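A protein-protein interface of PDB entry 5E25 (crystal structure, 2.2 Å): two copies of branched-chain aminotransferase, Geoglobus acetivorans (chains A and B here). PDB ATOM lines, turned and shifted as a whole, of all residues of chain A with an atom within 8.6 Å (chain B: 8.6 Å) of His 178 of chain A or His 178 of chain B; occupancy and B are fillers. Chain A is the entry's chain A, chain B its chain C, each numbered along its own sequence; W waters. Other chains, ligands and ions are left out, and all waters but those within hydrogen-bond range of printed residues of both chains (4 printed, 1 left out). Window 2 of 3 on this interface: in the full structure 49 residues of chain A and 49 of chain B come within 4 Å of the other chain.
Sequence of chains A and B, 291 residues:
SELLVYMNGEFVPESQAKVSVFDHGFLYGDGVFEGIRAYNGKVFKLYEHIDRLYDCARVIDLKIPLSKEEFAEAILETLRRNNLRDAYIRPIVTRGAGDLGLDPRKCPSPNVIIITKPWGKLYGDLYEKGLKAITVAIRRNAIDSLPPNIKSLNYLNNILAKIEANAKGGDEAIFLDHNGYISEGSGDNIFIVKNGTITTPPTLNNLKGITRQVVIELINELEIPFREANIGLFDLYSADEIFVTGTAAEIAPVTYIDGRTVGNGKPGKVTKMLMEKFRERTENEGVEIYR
The backbone NH (N) of Arg 139 of chain A is in hydrogen-bond range of the backbone carbonyl oxygen (O) of Asp 144 of chain B (2.7 Å). O of Asp 144 of chain A is in hydrogen-bond range of N of Arg 139 of chain B, 2.8 Å away. The side-chain hydroxyl (OG) of Ser 145 of chain A sits close to the backbone carbonyl oxygen (O) of Arg 139 of chain B (3.4 Å). The backbone carbonyl oxygen (O) of Arg 140 of chain B sits at hydrogen-bond distance from the side-chain hydroxyl (OG) of Ser 145 of chain A (3.2 Å).
The backbone carbonyl oxygen (O) of Asp 177 of chain A sits close to the guanidinium group (NE) of Arg 139 of chain A. O of Leu 176 of chain A lies within hydrogen-bond range of N of Arg 140 of chain A (2.9 Å). O of Asp 177 of chain B sits close to NE of Arg 139 of chain B (3.3 Å). The backbone NH (N) of Arg 140 of chain B sits at hydrogen-bond distance from the backbone carbonyl oxygen (O) of Leu 176 of chain B (2.8 Å).
Asp 144 of chain B touches Ile 138 of chain A (O to CD1, 3.5 Å). Arg 139 of chain A touches Ser 145 of chain B (O to CB, 3.2 Å). Ser 145 of chain B touches Arg 140 of chain A (CB to O, 3.7 Å). Ser 145 of chain B touches Asn 141 of chain A. CD1 of Ile 138 of chain B touches O of Ser 145 of chain A, at 3.4 Å. Asn 141 of chain B touches Ser 145 of chain A. His 178 of chain A touches His 178 of chain B (NE2 to CD2, 3.5 Å).
His 178 of chain A touches one residue of chain B. No residue of chain B comes within 4 Å of Asp 177 of chain A. No residue of chain A comes within 4 Å of Asp 177 of chain B. Printed residues of chain A within 4 Å of Arg 140 of chain B: Ser 145. Of the printed residues of chain B, Arg 140 of chain A touches Ser 145 (3.7 Å). Of the printed residues of chain A, Arg 139 of chain B touches Asp 144 (2.8 Å) and Ser 145 (3.4 Å). Printed residues of chain A within 4 Å of Asp 144 of chain B: Ile 138 (3.5 Å) and Arg 139 (2.7 Å). Of the printed residues of chain A, Asn 141 of chain B touches Ser 145 (3.8 Å). The nearest residue of chain A that does not touch His 178 of chain B is Asp 144 of chain A (4.6 Å).
Of the 18 printed residues of chain B, 7 touch a printed residue of chain A. Hydrophobic or aromatic side chains of chain B within 4 Å of the printed part of chain A: Ile 138 and His 178. Among the printed residues, 13 pairs touch across the chains. Among the printed residues, no Asp or Glu carboxylate lies within 4 Å of a Lys or Arg side-chain nitrogen of the other chain.
Arg 140 of chain A touches Ser 145 of chain B, and with the chains exchanged Ser 145 of chain A touches Arg 140 of chain B. His 178 of chain B touches its own counterpart, His 178 of chain A. Of the 13 pairs that touch across the chains among the printed residues, 13 have their exchanged pair printed and touching as well.
Water W4 bridges a ring nitrogen (ND1) of His 178 of chain B and the side-chain carboxylate (OD1) of Asp 144 of chain A. Water W3 lies within hydrogen-bond range of the side-chain amide nitrogen of Asn 141 of chain B, the side-chain amide nitrogen of Asn 141 of chain A and the side-chain hydroxyl of Ser 145 of chain B.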
ATOM      1  N   ILE A 138      22.508 -12.962  -9.799  1.00  0.00           N
ATOM      2  CA  ILE A 138      23.081 -14.087  -9.036  1.00  0.00           C
ATOM      3  C   ILE A 138      21.945 -14.771  -8.239  1.00  0.00           C
ATOM      4  O   ILE A 138      21.098 -14.079  -7.641  1.00  0.00           O
ATOM      5  CB  ILE A 138      24.241 -13.568  -8.113  1.00  0.00           C
ATOM      6  CG1 ILE A 138      25.029 -14.682  -7.471  1.00  0.00           C
ATOM      7  CG2 ILE A 138      23.756 -12.777  -6.908  1.00  0.00           C
ATOM      8  CD1 ILE A 138      26.144 -15.104  -8.333  1.00  0.00           C
ATOM      9  N   ARG A 139      21.898 -16.104  -8.226  1.00  0.00           N
ATOM     10  CA  ARG A 139      20.874 -16.820  -7.483  1.00  0.00           C
ATOM     11  C   ARG A 139      21.371 -17.186  -6.102  1.00  0.00           C
ATOM     12  O   ARG A 139      22.572 -17.165  -5.861  1.00  0.00           O
ATOM     13  CB  ARG A 139      20.482 -18.113  -8.212  1.00  0.00           C
ATOM     14  CG  ARG A 139      19.809 -17.857  -9.530  1.00  0.00           C
ATOM     15  CD  ARG A 139      18.469 -17.159  -9.266  1.00  0.00           C
ATOM     16  NE  ARG A 139      17.629 -17.124 -10.459  1.00  0.00           N
ATOM     17  CZ  ARG A 139      17.342 -16.062 -11.207  1.00  0.00           C
ATOM     18  NH1 ARG A 139      17.816 -14.826 -10.934  1.00  0.00           N
ATOM     19  NH2 ARG A 139      16.475 -16.228 -12.202  1.00  0.00           N
ATOM     20  N   ARG A 140      20.458 -17.541  -5.195  1.00  0.00           N
ATOM     21  CA  ARG A 140      20.863 -17.890  -3.807  1.00  0.00           C
ATOM     22  C   ARG A 140      21.587 -19.210  -3.863  1.00  0.00           C
ATOM     23  O   ARG A 140      21.198 -20.084  -4.673  1.00  0.00           O
ATOM     24  CB  ARG A 140      19.631 -18.069  -2.908  1.00  0.00           C
ATOM     25  CG  ARG A 140      19.966 -18.183  -1.398  1.00  0.00           C
ATOM     26  CD  ARG A 140      20.260 -16.766  -0.843  1.00  0.00           C
ATOM     27  NE  ARG A 140      20.409 -16.748   0.619  1.00  0.00           N
ATOM     28  CZ  ARG A 140      21.504 -17.072   1.313  1.00  0.00           C
ATOM     29  NH1 ARG A 140      22.673 -17.488   0.728  1.00  0.00           N
ATOM     30  NH2 ARG A 140      21.398 -17.030   2.631  1.00  0.00           N
ATOM     31  N   ASN A 141      22.569 -19.391  -2.971  1.00  0.00           N
ATOM     32  CA  ASN A 141      23.182 -20.698  -2.757  1.00  0.00           C
ATOM     33  C   ASN A 141      22.095 -21.792  -2.697  1.00  0.00           C
ATOM     34  O   ASN A 141      21.058 -21.611  -2.030  1.00  0.00           O
ATOM     35  CB  ASN A 141      23.914 -20.754  -1.407  1.00  0.00           C
ATOM     36  CG  ASN A 141      25.246 -19.999  -1.379  1.00  0.00           C
ATOM     37  OD1 ASN A 141      25.675 -19.507  -0.295  1.00  0.00           O
ATOM     38  ND2 ASN A 141      25.944 -19.971  -2.501  1.00  0.00           N
ATOM     39  N   ALA A 142      22.369 -22.939  -3.301  1.00  0.00           N
ATOM     40  CA  ALA A 142      21.346 -23.982  -3.470  1.00  0.00           C
ATOM     41  C   ALA A 142      21.335 -24.816  -2.206  1.00  0.00           C
ATOM     42  O   ALA A 142      22.400 -25.067  -1.605  1.00  0.00           O
ATOM     43  CB  ALA A 142      21.720 -24.874  -4.692  1.00  0.00           C
ATOM     44  N   ILE A 143      20.185 -25.384  -1.912  1.00  0.00           N
ATOM     45  CA  ILE A 143      19.951 -26.180  -0.708  1.00  0.00           C
ATOM     46  C   ILE A 143      20.748 -27.439  -0.694  1.00  0.00           C
ATOM     47  O   ILE A 143      20.960 -28.035   0.356  1.00  0.00           O
ATOM     48  CB  ILE A 143      18.441 -26.502  -0.515  1.00  0.00           C
ATOM     49  CG1 ILE A 143      17.833 -27.199  -1.764  1.00  0.00           C
ATOM     50  CG2 ILE A 143      17.766 -25.203  -0.141  1.00  0.00           C
ATOM     51  CD1 ILE A 143      16.392 -27.719  -1.550  1.00  0.00           C
ATOM     52  N   ASP A 144      21.279 -27.835  -1.833  1.00  0.00           N
ATOM     53  CA  ASP A 144      22.116 -29.005  -1.740  1.00  0.00           C
ATOM     54  C   ASP A 144      23.526 -28.778  -2.193  1.00  0.00           C
ATOM     55  O   ASP A 144      24.210 -29.760  -2.582  1.00  0.00           O
ATOM     56  CB  ASP A 144      21.478 -30.172  -2.486  1.00  0.00           C
ATOM     57  CG  ASP A 144      21.285 -29.895  -3.995  1.00  0.00           C
ATOM     58  OD1 ASP A 144      21.503 -28.784  -4.472  1.00  0.00           O
ATOM     59  OD2 ASP A 144      20.980 -30.863  -4.731  1.00  0.00           O
ATOM     60  N   SER A 145      23.957 -27.514  -2.150  1.00  0.00           N
ATOM     61  CA  SER A 145      25.380 -27.189  -2.356  1.00  0.00           C
ATOM     62  C   SER A 145      25.967 -26.543  -1.108  1.00  0.00           C
ATOM     63  O   SER A 145      27.057 -26.896  -0.625  1.00  0.00           O
ATOM     64  CB  SER A 145      25.528 -26.100  -3.445  1.00  0.00           C
ATOM     65  OG  SER A 145      25.116 -26.561  -4.665  1.00  0.00           O
ATOM     66  N   PHE A 175      17.369 -11.927  -3.814  1.00  0.00           N
ATOM     67  CA  PHE A 175      17.678 -13.209  -4.474  1.00  0.00           C
ATOM     68  C   PHE A 175      16.413 -13.938  -4.932  1.00  0.00           C
ATOM     69  O   PHE A 175      15.372 -13.924  -4.203  1.00  0.00           O
ATOM     70  CB  PHE A 175      18.284 -14.167  -3.496  1.00  0.00           C
ATOM     71  CG  PHE A 175      19.729 -13.970  -3.208  1.00  0.00           C
ATOM     72  CD1 PHE A 175      20.689 -14.280  -4.149  1.00  0.00           C
ATOM     73  CD2 PHE A 175      20.138 -13.607  -1.913  1.00  0.00           C
ATOM     74  CE1 PHE A 175      22.014 -14.200  -3.836  1.00  0.00           C
ATOM     75  CE2 PHE A 175      21.480 -13.522  -1.578  1.00  0.00           C
ATOM     76  CZ  PHE A 175      22.422 -13.872  -2.556  1.00  0.00           C
ATOM     77  N   LEU A 176      16.523 -14.610  -6.100  1.00  0.00           N
ATOM     78  CA  LEU A 176      15.683 -15.778  -6.427  1.00  0.00           C
ATOM     79  C   LEU A 176      16.520 -17.021  -6.177  1.00  0.00           C
ATOM     80  O   LEU A 176      17.717 -16.916  -6.046  1.00  0.00           O
ATOM     81  CB  LEU A 176      15.207 -15.820  -7.886  1.00  0.00           C
ATOM     82  CG  LEU A 176      14.582 -14.602  -8.594  1.00  0.00           C
ATOM     83  CD1 LEU A 176      13.625 -14.990  -9.705  1.00  0.00           C
ATOM     84  CD2 LEU A 176      13.975 -13.541  -7.742  1.00  0.00           C
ATOM     85  N   ASP A 177      15.897 -18.200  -6.127  1.00  0.00           N
ATOM     86  CA  ASP A 177      16.708 -19.388  -6.138  1.00  0.00           C
ATOM     87  C   ASP A 177      16.686 -19.957  -7.581  1.00  0.00           C
ATOM     88  O   ASP A 177      16.215 -19.322  -8.535  1.00  0.00           O
ATOM     89  CB  ASP A 177      16.187 -20.434  -5.111  1.00  0.00           C
ATOM     90  CG  ASP A 177      14.807 -21.004  -5.486  1.00  0.00           C
ATOM     91  OD1 ASP A 177      14.285 -20.718  -6.573  1.00  0.00           O
ATOM     92  OD2 ASP A 177      14.246 -21.788  -4.702  1.00  0.00           O
ATOM     93  N   HIS A 178      17.138 -21.185  -7.715  1.00  0.00           N
ATOM     94  CA  HIS A 178      17.390 -21.766  -9.008  1.00  0.00           C
ATOM     95  C   HIS A 178      16.066 -22.097  -9.728  1.00  0.00           C
ATOM     96  O   HIS A 178      16.044 -22.144 -10.934  1.00  0.00           O
ATOM     97  CB  HIS A 178      18.241 -23.018  -8.842  1.00  0.00           C
ATOM     98  CG  HIS A 178      18.547 -23.697 -10.136  1.00  0.00           C
ATOM     99  ND1 HIS A 178      19.529 -23.248 -10.997  1.00  0.00           N
ATOM    100  CD2 HIS A 178      17.956 -24.751 -10.750  1.00  0.00           C
ATOM    101  CE1 HIS A 178      19.559 -24.035 -12.063  1.00  0.00           C
ATOM    102  NE2 HIS A 178      18.603 -24.936 -11.950  1.00  0.00           N
ATOM    103  N   ASN A 179      15.003 -22.348  -8.968  1.00  0.00           N
ATOM    104  CA  ASN A 179      13.644 -22.594  -9.481  1.00  0.00           C
ATOM    105  C   ASN A 179      12.939 -21.350  -9.931  1.00  0.00           C
ATOM    106  O   ASN A 179      11.832 -21.429 -10.460  1.00  0.00           O
ATOM    107  CB  ASN A 179      12.771 -23.246  -8.374  1.00  0.00           C
ATOM    108  CG  ASN A 179      13.428 -24.493  -7.779  1.00  0.00           C
ATOM    109  OD1 ASN A 179      13.759 -24.536  -6.554  1.00  0.00           O
ATOM    110  ND2 ASN A 179      13.729 -25.467  -8.652  1.00  0.00           N
ATOM    111  N   GLY A 180      13.511 -20.194  -9.638  1.00  0.00           N
ATOM    112  CA  GLY A 180      12.818 -18.961  -9.974  1.00  0.00           C
ATOM    113  C   GLY A 180      11.958 -18.498  -8.809  1.00  0.00           C
ATOM    114  O   GLY A 180      11.183 -17.531  -8.947  1.00  0.00           O
ATOM    115  N   TYR A 181      12.008 -19.206  -7.679  1.00  0.00           N
ATOM    116  CA  TYR A 181      11.263 -18.695  -6.499  1.00  0.00           C
ATOM    117  C   TYR A 181      12.030 -17.536  -5.881  1.00  0.00           C
ATOM    118  O   TYR A 181      13.295 -17.572  -5.782  1.00  0.00           O
ATOM    119  CB  TYR A 181      11.117 -19.754  -5.414  1.00  0.00           C
ATOM    120  CG  TYR A 181      10.497 -21.065  -5.876  1.00  0.00           C
ATOM    121  CD1 TYR A 181       9.579 -21.106  -6.939  1.00  0.00           C
ATOM    122  CD2 TYR A 181      10.784 -22.255  -5.204  1.00  0.00           C
ATOM    123  CE1 TYR A 181       9.022 -22.302  -7.346  1.00  0.00           C
ATOM    124  CE2 TYR A 181      10.250 -23.472  -5.608  1.00  0.00           C
ATOM    125  CZ  TYR A 181       9.373 -23.500  -6.678  1.00  0.00           C
ATOM    126  OH  TYR A 181       8.784 -24.698  -7.017  1.00  0.00           O
ATOM    127  N   ILE A 182      11.292 -16.525  -5.431  1.00  0.00           N
ATOM    128  CA  ILE A 182      11.861 -15.520  -4.482  1.00  0.00           C
ATOM    129  C   ILE A 182      12.479 -16.211  -3.265  1.00  0.00           C
ATOM    130  O   ILE A 182      11.923 -17.190  -2.698  1.00  0.00           O
ATOM    131  CB  ILE A 182      10.831 -14.436  -4.029  1.00  0.00           C
ATOM    132  CG1 ILE A 182      10.092 -13.853  -5.240  1.00  0.00           C
ATOM    133  CG2 ILE A 182      11.493 -13.313  -3.197  1.00  0.00           C
ATOM    134  CD1 ILE A 182      10.989 -13.348  -6.363  1.00  0.00           C
ATOM    135  N   SER A 183      13.666 -15.749  -2.887  1.00  0.00           N
ATOM    136  CA  SER A 183      14.341 -16.355  -1.746  1.00  0.00           C
ATOM    137  C   SER A 183      14.302 -15.356  -0.562  1.00  0.00           C
ATOM    138  O   SER A 183      13.505 -15.557   0.368  1.00  0.00           O
ATOM    139  CB  SER A 183      15.731 -16.815  -2.150  1.00  0.00           C
ATOM    140  OG  SER A 183      16.604 -16.941  -1.031  1.00  0.00           O
ATOM    141  N   ASN A 205      14.684 -22.246   1.109  1.00  0.00           N
ATOM    142  CA  ASN A 205      15.665 -21.713   0.148  1.00  0.00           C
ATOM    143  C   ASN A 205      16.305 -20.419   0.667  1.00  0.00           C
ATOM    144  O   ASN A 205      17.015 -19.739  -0.070  1.00  0.00           O
ATOM    145  CB  ASN A 205      15.024 -21.528  -1.249  1.00  0.00           C
ATOM    146  CG  ASN A 205      14.131 -20.306  -1.326  1.00  0.00           C
ATOM    147  OD1 ASN A 205      14.088 -19.437  -0.408  1.00  0.00           O
ATOM    148  ND2 ASN A 205      13.545 -20.129  -2.480  1.00  0.00           N
ATOM    149  N   ILE B 138      26.241 -33.996  -1.562  1.00  0.00           N
ATOM    150  CA  ILE B 138      26.289 -32.536  -1.761  1.00  0.00           C
ATOM    151  C   ILE B 138      26.780 -32.203  -3.197  1.00  0.00           C
ATOM    152  O   ILE B 138      27.749 -32.828  -3.705  1.00  0.00           O
ATOM    153  CB  ILE B 138      27.102 -31.884  -0.612  1.00  0.00           C
ATOM    154  CG1 ILE B 138      26.957 -30.393  -0.550  1.00  0.00           C
ATOM    155  CG2 ILE B 138      28.602 -32.148  -0.706  1.00  0.00           C
ATOM    156  CD1 ILE B 138      25.862 -29.952   0.379  1.00  0.00           C
ATOM    157  N   ARG B 139      26.156 -31.224  -3.861  1.00  0.00           N
ATOM    158  CA  ARG B 139      26.540 -30.839  -5.254  1.00  0.00           C
ATOM    159  C   ARG B 139      27.511 -29.676  -5.260  1.00  0.00           C
ATOM    160  O   ARG B 139      27.572 -28.909  -4.279  1.00  0.00           O
ATOM    161  CB  ARG B 139      25.307 -30.465  -6.088  1.00  0.00           C
ATOM    162  CG  ARG B 139      24.354 -31.649  -6.358  1.00  0.00           C
ATOM    163  CD  ARG B 139      25.083 -32.742  -7.182  1.00  0.00           C
ATOM    164  NE  ARG B 139      24.175 -33.769  -7.710  1.00  0.00           N
ATOM    165  CZ  ARG B 139      24.099 -35.028  -7.308  1.00  0.00           C
ATOM    166  NH1 ARG B 139      24.929 -35.509  -6.359  1.00  0.00           N
ATOM    167  NH2 ARG B 139      23.249 -35.842  -7.948  1.00  0.00           N
ATOM    168  N   ARG B 140      28.280 -29.519  -6.342  1.00  0.00           N
ATOM    169  CA  ARG B 140      29.208 -28.394  -6.396  1.00  0.00           C
ATOM    170  C   ARG B 140      28.492 -27.056  -6.324  1.00  0.00           C
ATOM    171  O   ARG B 140      27.422 -26.918  -6.875  1.00  0.00           O
ATOM    172  CB  ARG B 140      30.089 -28.441  -7.691  1.00  0.00           C
ATOM    173  CG  ARG B 140      31.272 -27.456  -7.646  1.00  0.00           C
ATOM    174  CD  ARG B 140      32.365 -27.992  -6.686  1.00  0.00           C
ATOM    175  NE  ARG B 140      33.625 -27.249  -6.773  1.00  0.00           N
ATOM    176  CZ  ARG B 140      33.848 -26.100  -6.123  1.00  0.00           C
ATOM    177  NH1 ARG B 140      32.950 -25.570  -5.291  1.00  0.00           N
ATOM    178  NH2 ARG B 140      34.973 -25.465  -6.333  1.00  0.00           N
ATOM    179  N   ASN B 141      29.069 -26.025  -5.738  1.00  0.00           N
ATOM    180  CA  ASN B 141      28.466 -24.696  -5.831  1.00  0.00           C
ATOM    181  C   ASN B 141      28.097 -24.363  -7.306  1.00  0.00           C
ATOM    182  O   ASN B 141      28.895 -24.635  -8.258  1.00  0.00           O
ATOM    183  CB  ASN B 141      29.473 -23.609  -5.372  1.00  0.00           C
ATOM    184  CG  ASN B 141      29.693 -23.575  -3.863  1.00  0.00           C
ATOM    185  OD1 ASN B 141      30.783 -23.224  -3.379  1.00  0.00           O
ATOM    186  ND2 ASN B 141      28.688 -23.945  -3.123  1.00  0.00           N
ATOM    187  N   ALA B 142      26.954 -23.721  -7.499  1.00  0.00           N
ATOM    188  CA  ALA B 142      26.431 -23.559  -8.866  1.00  0.00           C
ATOM    189  C   ALA B 142      27.084 -22.328  -9.548  1.00  0.00           C
ATOM    190  O   ALA B 142      27.390 -21.273  -8.867  1.00  0.00           O
ATOM    191  CB  ALA B 142      24.930 -23.422  -8.846  1.00  0.00           C
ATOM    192  N   ILE B 143      27.225 -22.437 -10.882  1.00  0.00           N
ATOM    193  CA  ILE B 143      27.870 -21.334 -11.677  1.00  0.00           C
ATOM    194  C   ILE B 143      27.111 -20.009 -11.549  1.00  0.00           C
ATOM    195  O   ILE B 143      27.630 -18.943 -11.863  1.00  0.00           O
ATOM    196  CB  ILE B 143      28.092 -21.739 -13.175  1.00  0.00           C
ATOM    197  CG1 ILE B 143      26.747 -21.944 -13.889  1.00  0.00           C
ATOM    198  CG2 ILE B 143      29.001 -22.997 -13.301  1.00  0.00           C
ATOM    199  CD1 ILE B 143      26.924 -22.162 -15.389  1.00  0.00           C
ATOM    200  N   ASP B 144      25.856 -20.061 -11.155  1.00  0.00           N
ATOM    201  CA  ASP B 144      25.166 -18.815 -11.007  1.00  0.00           C
ATOM    202  C   ASP B 144      24.772 -18.439  -9.568  1.00  0.00           C
ATOM    203  O   ASP B 144      23.923 -17.550  -9.380  1.00  0.00           O
ATOM    204  CB  ASP B 144      23.961 -18.763 -11.939  1.00  0.00           C
ATOM    205  CG  ASP B 144      22.920 -19.746 -11.558  1.00  0.00           C
ATOM    206  OD1 ASP B 144      23.122 -20.532 -10.565  1.00  0.00           O
ATOM    207  OD2 ASP B 144      21.847 -19.658 -12.200  1.00  0.00           O
ATOM    208  N   SER B 145      25.437 -19.041  -8.584  1.00  0.00           N
ATOM    209  CA  SER B 145      25.226 -18.640  -7.201  1.00  0.00           C
ATOM    210  C   SER B 145      26.551 -18.307  -6.537  1.00  0.00           C
ATOM    211  O   SER B 145      26.705 -17.276  -5.923  1.00  0.00           O
ATOM    212  CB  SER B 145      24.417 -19.728  -6.454  1.00  0.00           C
ATOM    213  OG  SER B 145      25.246 -20.836  -6.209  1.00  0.00           O
ATOM    214  N   PHE B 175      32.478 -34.410  -6.531  1.00  0.00           N
ATOM    215  CA  PHE B 175      31.263 -33.647  -6.726  1.00  0.00           C
ATOM    216  C   PHE B 175      30.649 -33.893  -8.111  1.00  0.00           C
ATOM    217  O   PHE B 175      31.384 -34.095  -9.106  1.00  0.00           O
ATOM    218  CB  PHE B 175      31.618 -32.186  -6.796  1.00  0.00           C
ATOM    219  CG  PHE B 175      31.821 -31.516  -5.485  1.00  0.00           C
ATOM    220  CD1 PHE B 175      30.745 -31.244  -4.659  1.00  0.00           C
ATOM    221  CD2 PHE B 175      33.089 -31.019  -5.134  1.00  0.00           C
ATOM    222  CE1 PHE B 175      30.898 -30.456  -3.511  1.00  0.00           C
ATOM    223  CE2 PHE B 175      33.237 -30.243  -3.992  1.00  0.00           C
ATOM    224  CZ  PHE B 175      32.155 -29.965  -3.188  1.00  0.00           C
ATOM    225  N   LEU B 176      29.308 -33.862  -8.147  1.00  0.00           N
ATOM    226  CA  LEU B 176      28.553 -33.620  -9.361  1.00  0.00           C
ATOM    227  C   LEU B 176      27.983 -32.222  -9.223  1.00  0.00           C
ATOM    228  O   LEU B 176      27.984 -31.641  -8.145  1.00  0.00           O
ATOM    229  CB  LEU B 176      27.392 -34.651  -9.577  1.00  0.00           C
ATOM    230  CG  LEU B 176      27.423 -36.191  -9.492  1.00  0.00           C
ATOM    231  CD1 LEU B 176      26.321 -37.040 -10.148  1.00  0.00           C
ATOM    232  CD2 LEU B 176      28.779 -36.846  -9.523  1.00  0.00           C
ATOM    233  N   ASP B 177      27.507 -31.672 -10.321  1.00  0.00           N
ATOM    234  CA  ASP B 177      26.822 -30.396 -10.280  1.00  0.00           C
ATOM    235  C   ASP B 177      25.328 -30.689 -10.330  1.00  0.00           C
ATOM    236  O   ASP B 177      24.899 -31.826 -10.331  1.00  0.00           O
ATOM    237  CB  ASP B 177      27.295 -29.419 -11.424  1.00  0.00           C
ATOM    238  CG  ASP B 177      26.830 -29.846 -12.859  1.00  0.00           C
ATOM    239  OD1 ASP B 177      26.103 -30.867 -13.036  1.00  0.00           O
ATOM    240  OD2 ASP B 177      27.280 -29.182 -13.841  1.00  0.00           O
ATOM    241  N   HIS B 178      24.547 -29.643 -10.388  1.00  0.00           N
ATOM    242  CA  HIS B 178      23.095 -29.729 -10.400  1.00  0.00           C
ATOM    243  C   HIS B 178      22.523 -30.506 -11.597  1.00  0.00           C
ATOM    244  O   HIS B 178      21.458 -31.113 -11.463  1.00  0.00           O
ATOM    245  CB  HIS B 178      22.475 -28.312 -10.277  1.00  0.00           C
ATOM    246  CG  HIS B 178      20.971 -28.310 -10.124  1.00  0.00           C
ATOM    247  ND1 HIS B 178      20.333 -28.672  -8.951  1.00  0.00           N
ATOM    248  CD2 HIS B 178      19.984 -27.998 -11.005  1.00  0.00           C
ATOM    249  CE1 HIS B 178      19.025 -28.592  -9.121  1.00  0.00           C
ATOM    250  NE2 HIS B 178      18.784 -28.206 -10.365  1.00  0.00           N
ATOM    251  N   ASN B 179      23.208 -30.482 -12.746  1.00  0.00           N
ATOM    252  CA  ASN B 179      22.740 -31.198 -13.940  1.00  0.00           C
ATOM    253  C   ASN B 179      23.048 -32.664 -13.861  1.00  0.00           C
ATOM    254  O   ASN B 179      22.624 -33.423 -14.717  1.00  0.00           O
ATOM    255  CB  ASN B 179      23.449 -30.639 -15.179  1.00  0.00           C
ATOM    256  CG  ASN B 179      23.275 -29.138 -15.291  1.00  0.00           C
ATOM    257  OD1 ASN B 179      24.263 -28.396 -15.329  1.00  0.00           O
ATOM    258  ND2 ASN B 179      22.004 -28.668 -15.283  1.00  0.00           N
ATOM    259  N   GLY B 180      23.776 -33.097 -12.837  1.00  0.00           N
ATOM    260  CA  GLY B 180      24.235 -34.505 -12.848  1.00  0.00           C
ATOM    261  C   GLY B 180      25.580 -34.713 -13.543  1.00  0.00           C
ATOM    262  O   GLY B 180      26.043 -35.867 -13.653  1.00  0.00           O
ATOM    263  N   TYR B 181      26.230 -33.626 -14.001  1.00  0.00           N
ATOM    264  CA  TYR B 181      27.564 -33.771 -14.604  1.00  0.00           C
ATOM    265  C   TYR B 181      28.597 -33.980 -13.448  1.00  0.00           C
ATOM    266  O   TYR B 181      28.476 -33.365 -12.396  1.00  0.00           O
ATOM    267  CB  TYR B 181      27.976 -32.505 -15.397  1.00  0.00           C
ATOM    268  CG  TYR B 181      27.033 -32.100 -16.518  1.00  0.00           C
ATOM    269  CD1 TYR B 181      26.200 -33.061 -17.172  1.00  0.00           C
ATOM    270  CD2 TYR B 181      26.947 -30.762 -16.936  1.00  0.00           C
ATOM    271  CE1 TYR B 181      25.371 -32.707 -18.213  1.00  0.00           C
ATOM    272  CE2 TYR B 181      26.071 -30.392 -17.990  1.00  0.00           C
ATOM    273  CZ  TYR B 181      25.294 -31.375 -18.615  1.00  0.00           C
ATOM    274  OH  TYR B 181      24.405 -31.043 -19.650  1.00  0.00           O
ATOM    275  N   ILE B 182      29.587 -34.848 -13.671  1.00  0.00           N
ATOM    276  CA  ILE B 182      30.757 -34.865 -12.865  1.00  0.00           C
ATOM    277  C   ILE B 182      31.344 -33.442 -12.861  1.00  0.00           C
ATOM    278  O   ILE B 182      31.478 -32.791 -13.926  1.00  0.00           O
ATOM    279  CB  ILE B 182      31.791 -35.888 -13.403  1.00  0.00           C
ATOM    280  CG1 ILE B 182      31.202 -37.302 -13.548  1.00  0.00           C
ATOM    281  CG2 ILE B 182      33.041 -35.953 -12.517  1.00  0.00           C
ATOM    282  CD1 ILE B 182      30.280 -37.800 -12.419  1.00  0.00           C
ATOM    283  N   SER B 183      31.769 -32.987 -11.680  1.00  0.00           N
ATOM    284  CA  SER B 183      32.353 -31.695 -11.568  1.00  0.00           C
ATOM    285  C   SER B 183      33.858 -31.835 -11.358  1.00  0.00           C
ATOM    286  O   SER B 183      34.656 -31.557 -12.283  1.00  0.00           O
ATOM    287  CB  SER B 183      31.607 -30.808 -10.478  1.00  0.00           C
ATOM    288  OG  SER B 183      32.416 -29.677 -10.152  1.00  0.00           O
ATOM    289  N   ASN B 205      31.844 -25.944 -14.587  1.00  0.00           N
ATOM    290  CA  ASN B 205      31.186 -26.295 -13.311  1.00  0.00           C
ATOM    291  C   ASN B 205      32.227 -26.683 -12.233  1.00  0.00           C
ATOM    292  O   ASN B 205      31.863 -27.216 -11.156  1.00  0.00           O
ATOM    293  CB  ASN B 205      30.219 -27.455 -13.495  1.00  0.00           C
ATOM    294  CG  ASN B 205      30.951 -28.794 -13.681  1.00  0.00           C
ATOM    295  OD1 ASN B 205      32.186 -28.850 -13.586  1.00  0.00           O
ATOM    296  ND2 ASN B 205      30.189 -29.889 -13.948  1.00  0.00           N
HETATM  297  O   HOH W   1      24.841 -23.299  -5.367  1.00  0.00           O
HETATM  298  O   HOH W   2      16.744 -27.614 -12.957  1.00  0.00           O
HETATM  299  O   HOH W   3      26.574 -22.420  -3.530  1.00  0.00           O
HETATM  300  O   HOH W   4      21.988 -29.093  -7.081  1.00  0.00           O
